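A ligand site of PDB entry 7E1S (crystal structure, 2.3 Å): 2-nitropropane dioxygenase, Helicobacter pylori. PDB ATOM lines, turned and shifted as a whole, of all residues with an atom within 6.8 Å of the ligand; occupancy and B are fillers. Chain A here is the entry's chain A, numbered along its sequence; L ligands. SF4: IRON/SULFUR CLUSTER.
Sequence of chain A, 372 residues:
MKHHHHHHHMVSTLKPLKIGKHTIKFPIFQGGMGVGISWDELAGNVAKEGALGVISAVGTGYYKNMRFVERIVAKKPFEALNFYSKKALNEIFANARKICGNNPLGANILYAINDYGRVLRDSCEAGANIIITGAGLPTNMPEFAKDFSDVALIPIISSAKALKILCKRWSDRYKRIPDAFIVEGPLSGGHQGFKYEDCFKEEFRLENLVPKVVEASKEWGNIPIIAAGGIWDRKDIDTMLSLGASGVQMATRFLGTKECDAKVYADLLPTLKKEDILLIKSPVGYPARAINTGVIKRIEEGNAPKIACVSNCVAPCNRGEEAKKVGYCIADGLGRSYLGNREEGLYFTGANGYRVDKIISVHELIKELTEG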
ATOM      1  N   PHE A  83      -5.295 -27.113 -15.141  1.00  0.00           N
ATOM      2  CA  PHE A  83      -4.184 -26.583 -14.356  1.00  0.00           C
ATOM      3  C   PHE A  83      -4.499 -26.608 -12.863  1.00  0.00           C
ATOM      4  O   PHE A  83      -3.695 -27.078 -12.050  1.00  0.00           O
ATOM      5  CB  PHE A  83      -3.888 -25.172 -14.839  1.00  0.00           C
ATOM      6  CG  PHE A  83      -2.654 -24.546 -14.266  1.00  0.00           C
ATOM      7  CD1 PHE A  83      -1.398 -24.969 -14.671  1.00  0.00           C
ATOM      8  CD2 PHE A  83      -2.751 -23.503 -13.357  1.00  0.00           C
ATOM      9  CE1 PHE A  83      -0.263 -24.371 -14.178  1.00  0.00           C
ATOM     10  CE2 PHE A  83      -1.645 -22.893 -12.862  1.00  0.00           C
ATOM     11  CZ  PHE A  83      -0.382 -23.331 -13.263  1.00  0.00           C
ATOM     12  N   TYR A  84      -5.692 -26.127 -12.489  1.00  0.00           N
ATOM     13  CA  TYR A  84      -6.189 -26.181 -11.106  1.00  0.00           C
ATOM     14  C   TYR A  84      -7.111 -27.385 -10.977  1.00  0.00           C
ATOM     15  O   TYR A  84      -8.339 -27.265 -10.991  1.00  0.00           O
ATOM     16  CB  TYR A  84      -6.919 -24.886 -10.731  1.00  0.00           C
ATOM     17  CG  TYR A  84      -6.138 -23.634 -11.043  1.00  0.00           C
ATOM     18  CD1 TYR A  84      -5.011 -23.300 -10.312  1.00  0.00           C
ATOM     19  CD2 TYR A  84      -6.516 -22.781 -12.089  1.00  0.00           C
ATOM     20  CE1 TYR A  84      -4.298 -22.161 -10.589  1.00  0.00           C
ATOM     21  CE2 TYR A  84      -5.808 -21.630 -12.360  1.00  0.00           C
ATOM     22  CZ  TYR A  84      -4.685 -21.332 -11.608  1.00  0.00           C
ATOM     23  OH  TYR A  84      -3.942 -20.200 -11.864  1.00  0.00           O
ATOM     24  N   ASN A 114      -7.437 -17.593 -12.625  1.00  0.00           N
ATOM     25  CA  ASN A 114      -8.751 -17.861 -13.153  1.00  0.00           C
ATOM     26  C   ASN A 114      -9.392 -18.995 -12.364  1.00  0.00           C
ATOM     27  O   ASN A 114      -8.691 -19.848 -11.816  1.00  0.00           O
ATOM     28  CB  ASN A 114      -8.682 -18.210 -14.642  1.00  0.00           C
ATOM     29  CG  ASN A 114      -8.368 -17.007 -15.505  1.00  0.00           C
ATOM     30  OD1 ASN A 114      -8.856 -15.907 -15.264  1.00  0.00           O
ATOM     31  ND2 ASN A 114      -7.506 -17.213 -16.496  1.00  0.00           N
ATOM     32  N   PRO A 283       4.058 -12.016 -15.386  1.00  0.00           N
ATOM     33  CA  PRO A 283       2.701 -11.863 -15.969  1.00  0.00           C
ATOM     34  C   PRO A 283       1.628 -11.626 -14.913  1.00  0.00           C
ATOM     35  O   PRO A 283       0.546 -11.126 -15.253  1.00  0.00           O
ATOM     36  CB  PRO A 283       2.475 -13.201 -16.688  1.00  0.00           C
ATOM     37  CG  PRO A 283       3.820 -13.817 -16.814  1.00  0.00           C
ATOM     38  CD  PRO A 283       4.603 -13.351 -15.631  1.00  0.00           C
ATOM     39  N   VAL A 284       1.861 -12.001 -13.648  1.00  0.00           N
ATOM     40  CA  VAL A 284       0.845 -11.793 -12.620  1.00  0.00           C
ATOM     41  C   VAL A 284       0.627 -10.298 -12.372  1.00  0.00           C
ATOM     42  O   VAL A 284      -0.455  -9.895 -11.917  1.00  0.00           O
ATOM     43  CB  VAL A 284       1.212 -12.516 -11.302  1.00  0.00           C
ATOM     44  CG1 VAL A 284       0.064 -12.455 -10.309  1.00  0.00           C
ATOM     45  CG2 VAL A 284       1.570 -13.978 -11.568  1.00  0.00           C
ATOM     46  N   ILE A 307       6.147 -18.974 -26.076  1.00  0.00           N
ATOM     47  CA  ILE A 307       5.016 -18.594 -25.238  1.00  0.00           C
ATOM     48  C   ILE A 307       3.745 -18.815 -26.050  1.00  0.00           C
ATOM     49  O   ILE A 307       3.497 -18.120 -27.038  1.00  0.00           O
ATOM     50  CB  ILE A 307       5.135 -17.124 -24.792  1.00  0.00           C
ATOM     51  CG1 ILE A 307       6.212 -16.972 -23.714  1.00  0.00           C
ATOM     52  CG2 ILE A 307       3.782 -16.609 -24.313  1.00  0.00           C
ATOM     53  CD1 ILE A 307       6.797 -15.569 -23.645  1.00  0.00           C
ATOM     54  N   ALA A 308       2.927 -19.783 -25.645  1.00  0.00           N
ATOM     55  CA  ALA A 308       1.619 -20.021 -26.263  1.00  0.00           C
ATOM     56  C   ALA A 308       0.648 -20.449 -25.171  1.00  0.00           C
ATOM     57  O   ALA A 308       0.672 -21.605 -24.749  1.00  0.00           O
ATOM     58  CB  ALA A 308       1.714 -21.089 -27.347  1.00  0.00           C
ATOM     59  N   CYS A 309      -0.207 -19.518 -24.725  1.00  0.00           N
ATOM     60  CA  CYS A 309      -1.019 -19.705 -23.527  1.00  0.00           C
ATOM     61  C   CYS A 309      -1.898 -20.956 -23.606  1.00  0.00           C
ATOM     62  O   CYS A 309      -2.919 -20.963 -24.316  1.00  0.00           O
ATOM     63  CB  CYS A 309      -1.900 -18.459 -23.280  1.00  0.00           C
ATOM     64  SG  CYS A 309      -2.887 -18.454 -21.681  1.00  0.00           S
ATOM     65  N   VAL A 310      -1.536 -22.008 -22.872  1.00  0.00           N
ATOM     66  CA  VAL A 310      -2.325 -23.238 -22.782  1.00  0.00           C
ATOM     67  C   VAL A 310      -3.086 -23.332 -21.454  1.00  0.00           C
ATOM     68  O   VAL A 310      -4.295 -23.573 -21.439  1.00  0.00           O
ATOM     69  CB  VAL A 310      -1.407 -24.472 -23.003  1.00  0.00           C
ATOM     70  CG1 VAL A 310      -2.155 -25.758 -22.747  1.00  0.00           C
ATOM     71  CG2 VAL A 310      -0.814 -24.456 -24.397  1.00  0.00           C
ATOM     72  N   SER A 311      -2.396 -23.115 -20.323  1.00  0.00           N
ATOM     73  CA  SER A 311      -3.019 -23.288 -19.011  1.00  0.00           C
ATOM     74  C   SER A 311      -3.925 -22.126 -18.598  1.00  0.00           C
ATOM     75  O   SER A 311      -4.882 -22.347 -17.845  1.00  0.00           O
ATOM     76  CB  SER A 311      -1.942 -23.500 -17.944  1.00  0.00           C
ATOM     77  OG  SER A 311      -1.305 -24.760 -18.111  1.00  0.00           O
ATOM     78  N   ASN A 312      -3.653 -20.908 -19.066  1.00  0.00           N
ATOM     79  CA  ASN A 312      -4.412 -19.693 -18.723  1.00  0.00           C
ATOM     80  C   ASN A 312      -4.558 -19.559 -17.223  1.00  0.00           C
ATOM     81  O   ASN A 312      -5.659 -19.497 -16.654  1.00  0.00           O
ATOM     82  CB  ASN A 312      -5.761 -19.690 -19.440  1.00  0.00           C
ATOM     83  CG  ASN A 312      -6.487 -18.372 -19.313  1.00  0.00           C
ATOM     84  OD1 ASN A 312      -5.892 -17.281 -19.217  1.00  0.00           O
ATOM     85  ND2 ASN A 312      -7.803 -18.455 -19.297  1.00  0.00           N
ATOM     86  N   CYS A 313      -3.392 -19.478 -16.574  1.00  0.00           N
ATOM     87  CA  CYS A 313      -3.326 -19.601 -15.122  1.00  0.00           C
ATOM     88  C   CYS A 313      -3.926 -18.392 -14.430  1.00  0.00           C
ATOM     89  O   CYS A 313      -4.757 -18.536 -13.521  1.00  0.00           O
ATOM     90  CB  CYS A 313      -1.867 -19.856 -14.674  1.00  0.00           C
ATOM     91  SG  CYS A 313      -0.662 -18.536 -15.057  1.00  0.00           S
ATOM     92  N   VAL A 314      -3.551 -17.176 -14.842  1.00  0.00           N
ATOM     93  CA  VAL A 314      -3.925 -15.970 -14.121  1.00  0.00           C
ATOM     94  C   VAL A 314      -4.611 -14.969 -15.041  1.00  0.00           C
ATOM     95  O   VAL A 314      -4.231 -14.812 -16.218  1.00  0.00           O
ATOM     96  CB  VAL A 314      -2.701 -15.335 -13.421  1.00  0.00           C
ATOM     97  CG1 VAL A 314      -2.190 -16.231 -12.298  1.00  0.00           C
ATOM     98  CG2 VAL A 314      -1.612 -15.013 -14.421  1.00  0.00           C
ATOM     99  N   ALA A 315      -5.608 -14.275 -14.506  1.00  0.00           N
ATOM    100  CA  ALA A 315      -6.365 -13.300 -15.281  1.00  0.00           C
ATOM    101  C   ALA A 315      -5.563 -12.080 -15.733  1.00  0.00           C
ATOM    102  O   ALA A 315      -5.760 -11.649 -16.877  1.00  0.00           O
ATOM    103  CB  ALA A 315      -7.590 -12.862 -14.470  1.00  0.00           C
ATOM    104  N   PRO A 316      -4.664 -11.485 -14.937  1.00  0.00           N
ATOM    105  CA  PRO A 316      -3.954 -10.282 -15.433  1.00  0.00           C
ATOM    106  C   PRO A 316      -3.130 -10.518 -16.701  1.00  0.00           C
ATOM    107  O   PRO A 316      -2.711  -9.536 -17.334  1.00  0.00           O
ATOM    108  CB  PRO A 316      -3.032  -9.910 -14.249  1.00  0.00           C
ATOM    109  CG  PRO A 316      -3.709 -10.465 -13.060  1.00  0.00           C
ATOM    110  CD  PRO A 316      -4.320 -11.753 -13.522  1.00  0.00           C
ATOM    111  N   CYS A 317      -2.869 -11.776 -17.085  1.00  0.00           N
ATOM    112  CA  CYS A 317      -1.981 -12.020 -18.198  1.00  0.00           C
ATOM    113  C   CYS A 317      -2.672 -11.758 -19.520  1.00  0.00           C
ATOM    114  O   CYS A 317      -2.014 -11.421 -20.505  1.00  0.00           O
ATOM    115  CB  CYS A 317      -1.444 -13.461 -18.169  1.00  0.00           C
ATOM    116  SG  CYS A 317      -0.160 -13.862 -19.482  1.00  0.00           S
ATOM    117  N   ASN A 318      -4.011 -11.855 -19.546  1.00  0.00           N
ATOM    118  CA  ASN A 318      -4.767 -11.836 -20.804  1.00  0.00           C
ATOM    119  C   ASN A 318      -4.143 -12.783 -21.805  1.00  0.00           C
ATOM    120  O   ASN A 318      -4.053 -12.454 -22.997  1.00  0.00           O
ATOM    121  CB  ASN A 318      -4.853 -10.447 -21.443  1.00  0.00           C
ATOM    122  CG  ASN A 318      -5.104  -9.343 -20.465  1.00  0.00           C
ATOM    123  OD1 ASN A 318      -4.300  -8.408 -20.368  1.00  0.00           O
ATOM    124  ND2 ASN A 318      -6.258  -9.366 -19.767  1.00  0.00           N
ATOM    125  N   ARG A 319      -4.002 -13.988 -21.392  1.00  0.00           N
ATOM    126  CA  ARG A 319      -3.606 -15.142 -22.233  1.00  0.00           C
ATOM    127  C   ARG A 319      -2.368 -14.985 -23.129  1.00  0.00           C
ATOM    128  O   ARG A 319      -2.515 -15.355 -24.228  1.00  0.00           O
ATOM    129  CB  ARG A 319      -4.845 -15.550 -23.013  1.00  0.00           C
ATOM    130  CG  ARG A 319      -6.039 -15.749 -22.112  1.00  0.00           C
ATOM    131  CD  ARG A 319      -7.138 -16.310 -22.924  1.00  0.00           C
ATOM    132  NE  ARG A 319      -8.251 -15.424 -22.759  1.00  0.00           N
ATOM    133  CZ  ARG A 319      -8.301 -14.143 -23.095  1.00  0.00           C
ATOM    134  NH1 ARG A 319      -7.258 -13.526 -23.608  1.00  0.00           N
ATOM    135  NH2 ARG A 319      -9.385 -13.465 -22.860  1.00  0.00           N
ATOM    136  N   GLY A 320      -1.221 -14.513 -22.642  1.00  0.00           N
ATOM    137  CA  GLY A 320      -0.024 -14.288 -23.423  1.00  0.00           C
ATOM    138  C   GLY A 320       0.376 -12.833 -23.478  1.00  0.00           C
ATOM    139  O   GLY A 320       1.555 -12.553 -23.702  1.00  0.00           O
ATOM    140  N   GLU A 321      -0.555 -11.909 -23.288  1.00  0.00           N
ATOM    141  CA  GLU A 321      -0.176 -10.523 -23.528  1.00  0.00           C
ATOM    142  C   GLU A 321       0.915 -10.090 -22.584  1.00  0.00           C
ATOM    143  O   GLU A 321       1.943  -9.565 -23.004  1.00  0.00           O
ATOM    144  CB  GLU A 321      -1.382  -9.614 -23.437  1.00  0.00           C
ATOM    145  CG  GLU A 321      -2.428  -9.989 -24.430  1.00  0.00           C
ATOM    146  CD  GLU A 321      -3.539  -8.972 -24.494  1.00  0.00           C
ATOM    147  OE1 GLU A 321      -4.525  -9.262 -25.197  1.00  0.00           O
ATOM    148  OE2 GLU A 321      -3.401  -7.893 -23.887  1.00  0.00           O
ATOM    149  N   GLU A 322       0.727 -10.368 -21.288  1.00  0.00           N
ATOM    150  CA  GLU A 322       1.762  -9.980 -20.332  1.00  0.00           C
ATOM    151  C   GLU A 322       2.935 -10.956 -20.316  1.00  0.00           C
ATOM    152  O   GLU A 322       4.065 -10.531 -20.073  1.00  0.00           O
ATOM    153  CB  GLU A 322       1.115  -9.823 -18.959  1.00  0.00           C
ATOM    154  CG  GLU A 322      -0.026  -8.834 -18.992  1.00  0.00           C
ATOM    155  CD  GLU A 322       0.403  -7.482 -19.514  1.00  0.00           C
ATOM    156  OE1 GLU A 322       1.556  -7.069 -19.261  1.00  0.00           O
ATOM    157  OE2 GLU A 322      -0.427  -6.841 -20.201  1.00  0.00           O
ATOM    158  N   ALA A 323       2.691 -12.235 -20.587  1.00  0.00           N
ATOM    159  CA  ALA A 323       3.766 -13.216 -20.609  1.00  0.00           C
ATOM    160  C   ALA A 323       4.739 -12.940 -21.768  1.00  0.00           C
ATOM    161  O   ALA A 323       5.960 -12.933 -21.573  1.00  0.00           O
ATOM    162  CB  ALA A 323       3.179 -14.621 -20.711  1.00  0.00           C
ATOM    163  N   LYS A 324       4.196 -12.673 -22.956  1.00  0.00           N
ATOM    164  CA  LYS A 324       5.053 -12.311 -24.081  1.00  0.00           C
ATOM    165  C   LYS A 324       5.821 -11.023 -23.811  1.00  0.00           C
ATOM    166  O   LYS A 324       6.933 -10.861 -24.313  1.00  0.00           O
ATOM    167  CB  LYS A 324       4.208 -12.161 -25.353  1.00  0.00           C
ATOM    168  CG  LYS A 324       3.672 -13.455 -25.928  1.00  0.00           C
ATOM    169  CD  LYS A 324       2.883 -13.161 -27.208  1.00  0.00           C
ATOM    170  CE  LYS A 324       1.423 -12.849 -26.904  1.00  0.00           C
ATOM    171  NZ  LYS A 324       0.761 -11.956 -27.926  1.00  0.00           N
ATOM    172  N   TYR A 328       8.289 -14.839 -20.333  1.00  0.00           N
ATOM    173  CA  TYR A 328       8.059 -16.200 -19.897  1.00  0.00           C
ATOM    174  C   TYR A 328       6.605 -16.383 -19.487  1.00  0.00           C
ATOM    175  O   TYR A 328       5.931 -15.429 -19.088  1.00  0.00           O
ATOM    176  CB  TYR A 328       9.001 -16.566 -18.734  1.00  0.00           C
ATOM    177  CG  TYR A 328       8.763 -15.773 -17.452  1.00  0.00           C
ATOM    178  CD1 TYR A 328       9.390 -14.540 -17.259  1.00  0.00           C
ATOM    179  CD2 TYR A 328       7.913 -16.232 -16.452  1.00  0.00           C
ATOM    180  CE1 TYR A 328       9.181 -13.794 -16.114  1.00  0.00           C
ATOM    181  CE2 TYR A 328       7.689 -15.483 -15.291  1.00  0.00           C
ATOM    182  CZ  TYR A 328       8.333 -14.261 -15.129  1.00  0.00           C
ATOM    183  OH  TYR A 328       8.142 -13.509 -13.999  1.00  0.00           O
ATOM    184  N   CYS A 329       6.137 -17.606 -19.636  1.00  0.00           N
ATOM    185  CA  CYS A 329       4.889 -18.092 -19.068  1.00  0.00           C
ATOM    186  C   CYS A 329       5.154 -18.646 -17.668  1.00  0.00           C
ATOM    187  O   CYS A 329       5.946 -19.581 -17.509  1.00  0.00           O
ATOM    188  CB  CYS A 329       4.335 -19.204 -19.959  1.00  0.00           C
ATOM    189  SG  CYS A 329       2.920 -20.023 -19.284  1.00  0.00           S
ATOM    190  N   ILE A 330       4.477 -18.079 -16.656  1.00  0.00           N
ATOM    191  CA  ILE A 330       4.799 -18.481 -15.295  1.00  0.00           C
ATOM    192  C   ILE A 330       4.212 -19.859 -14.989  1.00  0.00           C
ATOM    193  O   ILE A 330       4.815 -20.632 -14.226  1.00  0.00           O
ATOM    194  CB  ILE A 330       4.346 -17.423 -14.272  1.00  0.00           C
ATOM    195  CG1 ILE A 330       5.003 -17.669 -12.912  1.00  0.00           C
ATOM    196  CG2 ILE A 330       2.801 -17.372 -14.126  1.00  0.00           C
ATOM    197  CD1 ILE A 330       4.677 -16.578 -11.882  1.00  0.00           C
ATOM    198  N   ALA A 331       3.068 -20.220 -15.581  1.00  0.00           N
ATOM    199  CA  ALA A 331       2.546 -21.559 -15.368  1.00  0.00           C
ATOM    200  C   ALA A 331       3.488 -22.610 -15.940  1.00  0.00           C
ATOM    201  O   ALA A 331       3.794 -23.617 -15.294  1.00  0.00           O
ATOM    202  CB  ALA A 331       1.159 -21.691 -16.013  1.00  0.00           C
ATOM    203  N   ASP A 332       3.979 -22.368 -17.164  1.00  0.00           N
ATOM    204  CA  ASP A 332       4.899 -23.293 -17.805  1.00  0.00           C
ATOM    205  C   ASP A 332       6.231 -23.323 -17.082  1.00  0.00           C
ATOM    206  O   ASP A 332       6.808 -24.395 -16.896  1.00  0.00           O
ATOM    207  CB  ASP A 332       5.119 -22.897 -19.278  1.00  0.00           C
ATOM    208  CG  ASP A 332       3.832 -22.960 -20.116  1.00  0.00           C
ATOM    209  OD1 ASP A 332       2.782 -23.429 -19.657  1.00  0.00           O
ATOM    210  OD2 ASP A 332       3.875 -22.428 -21.230  1.00  0.00           O
HETATM  211 FE1  SF4 L   1      -1.285 -18.378 -20.004  1.00  0.00          FE
HETATM  212 FE2  SF4 L   1      -0.075 -16.103 -19.198  1.00  0.00          FE
HETATM  213 FE3  SF4 L   1       1.273 -18.457 -19.140  1.00  0.00          FE
HETATM  214 FE4  SF4 L   1      -0.679 -18.043 -17.320  1.00  0.00          FE
HETATM  215  S1  SF4 L   1       1.265 -16.856 -17.545  1.00  0.00           S
HETATM  216  S2  SF4 L   1      -0.374 -19.913 -18.595  1.00  0.00           S
HETATM  217  S3  SF4 L   1      -2.174 -16.820 -18.554  1.00  0.00           S
HETATM  218  S4  SF4 L   1       0.499 -17.363 -21.007  1.00  0.00           S
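S2 of the ligand sits close to N of Asn 312, 3.5 Å away.
The backbone NH (N) of Gly 320 lies close to a sulfur (S4) of the ligand (3.7 Å).
The backbone NH (N) of Cys 313 lies close to a sulfur (S3) of the ligand.
An iron atom (FE3) of the ligand is bound by the side-chain sulfur (SG) of Cys 329 (2.3 Å).
SG of Cys 317 is bound to FE2 of the ligand (2.3 Å).
SG of Cys 313 is bound to FE4 of the ligand, at 2.3 Å.
A sulfur (S1) of the ligand lies close to the backbone NH (N) of Ile 330, 3.6 Å away.
The side-chain sulfur (SG) of Cys 309 binds an iron atom (FE1) of the ligand, 2.3 Å away.
O of Val 314 lies close to S3 of the ligand (3.7 Å).
CB of Pro 283 touches S1 of the ligand (3.9 Å).
CB of Ser 311 touches S2 of the ligand, at 3.97 Å.
Ala 323 touches the ligand (CB to S4, 3.8 Å).
CB of Ala 331 touches S2 of the ligand, 3.5 Å away.
Within 4 Å of the ligand: Pro 283, Cys 309, Ser 311, Asn 312, Cys 313, Val 314, Cys 317, Gly 320, Ala 323, Cys 329, Ile 330 and Ala 331.
The nearest printed residue that does not touch the ligand is Arg 319 (4.3 Å).
The side-chain sulfur (SG) of Cys 309 sits close to the backbone NH (N) of Asn 312 (3.7 Å).
The side-chain sulfur of Cys 329 lies close to the side-chain carboxylate of Asp 332 (3.2 Å).
O of Ala 323 sits at hydrogen-bond distance from N of Tyr 328 (3.3 Å).
The side-chain sulfur (SG) of Cys 317 sits close to the backbone NH (N) of Gly 320, 3.4 Å away.
N of Glu 322 lies within hydrogen-bond range of O of Cys 317 (3.0 Å).
The backbone NH of Ala 323 sits close to the side-chain sulfur of Cys 317 (3.5 Å).
O of Cys 313 is in hydrogen-bond range of OH of Tyr 84.
The backbone NH (N) of Asn 114 lies within hydrogen-bond range of the backbone carbonyl oxygen (O) of Cys 313.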
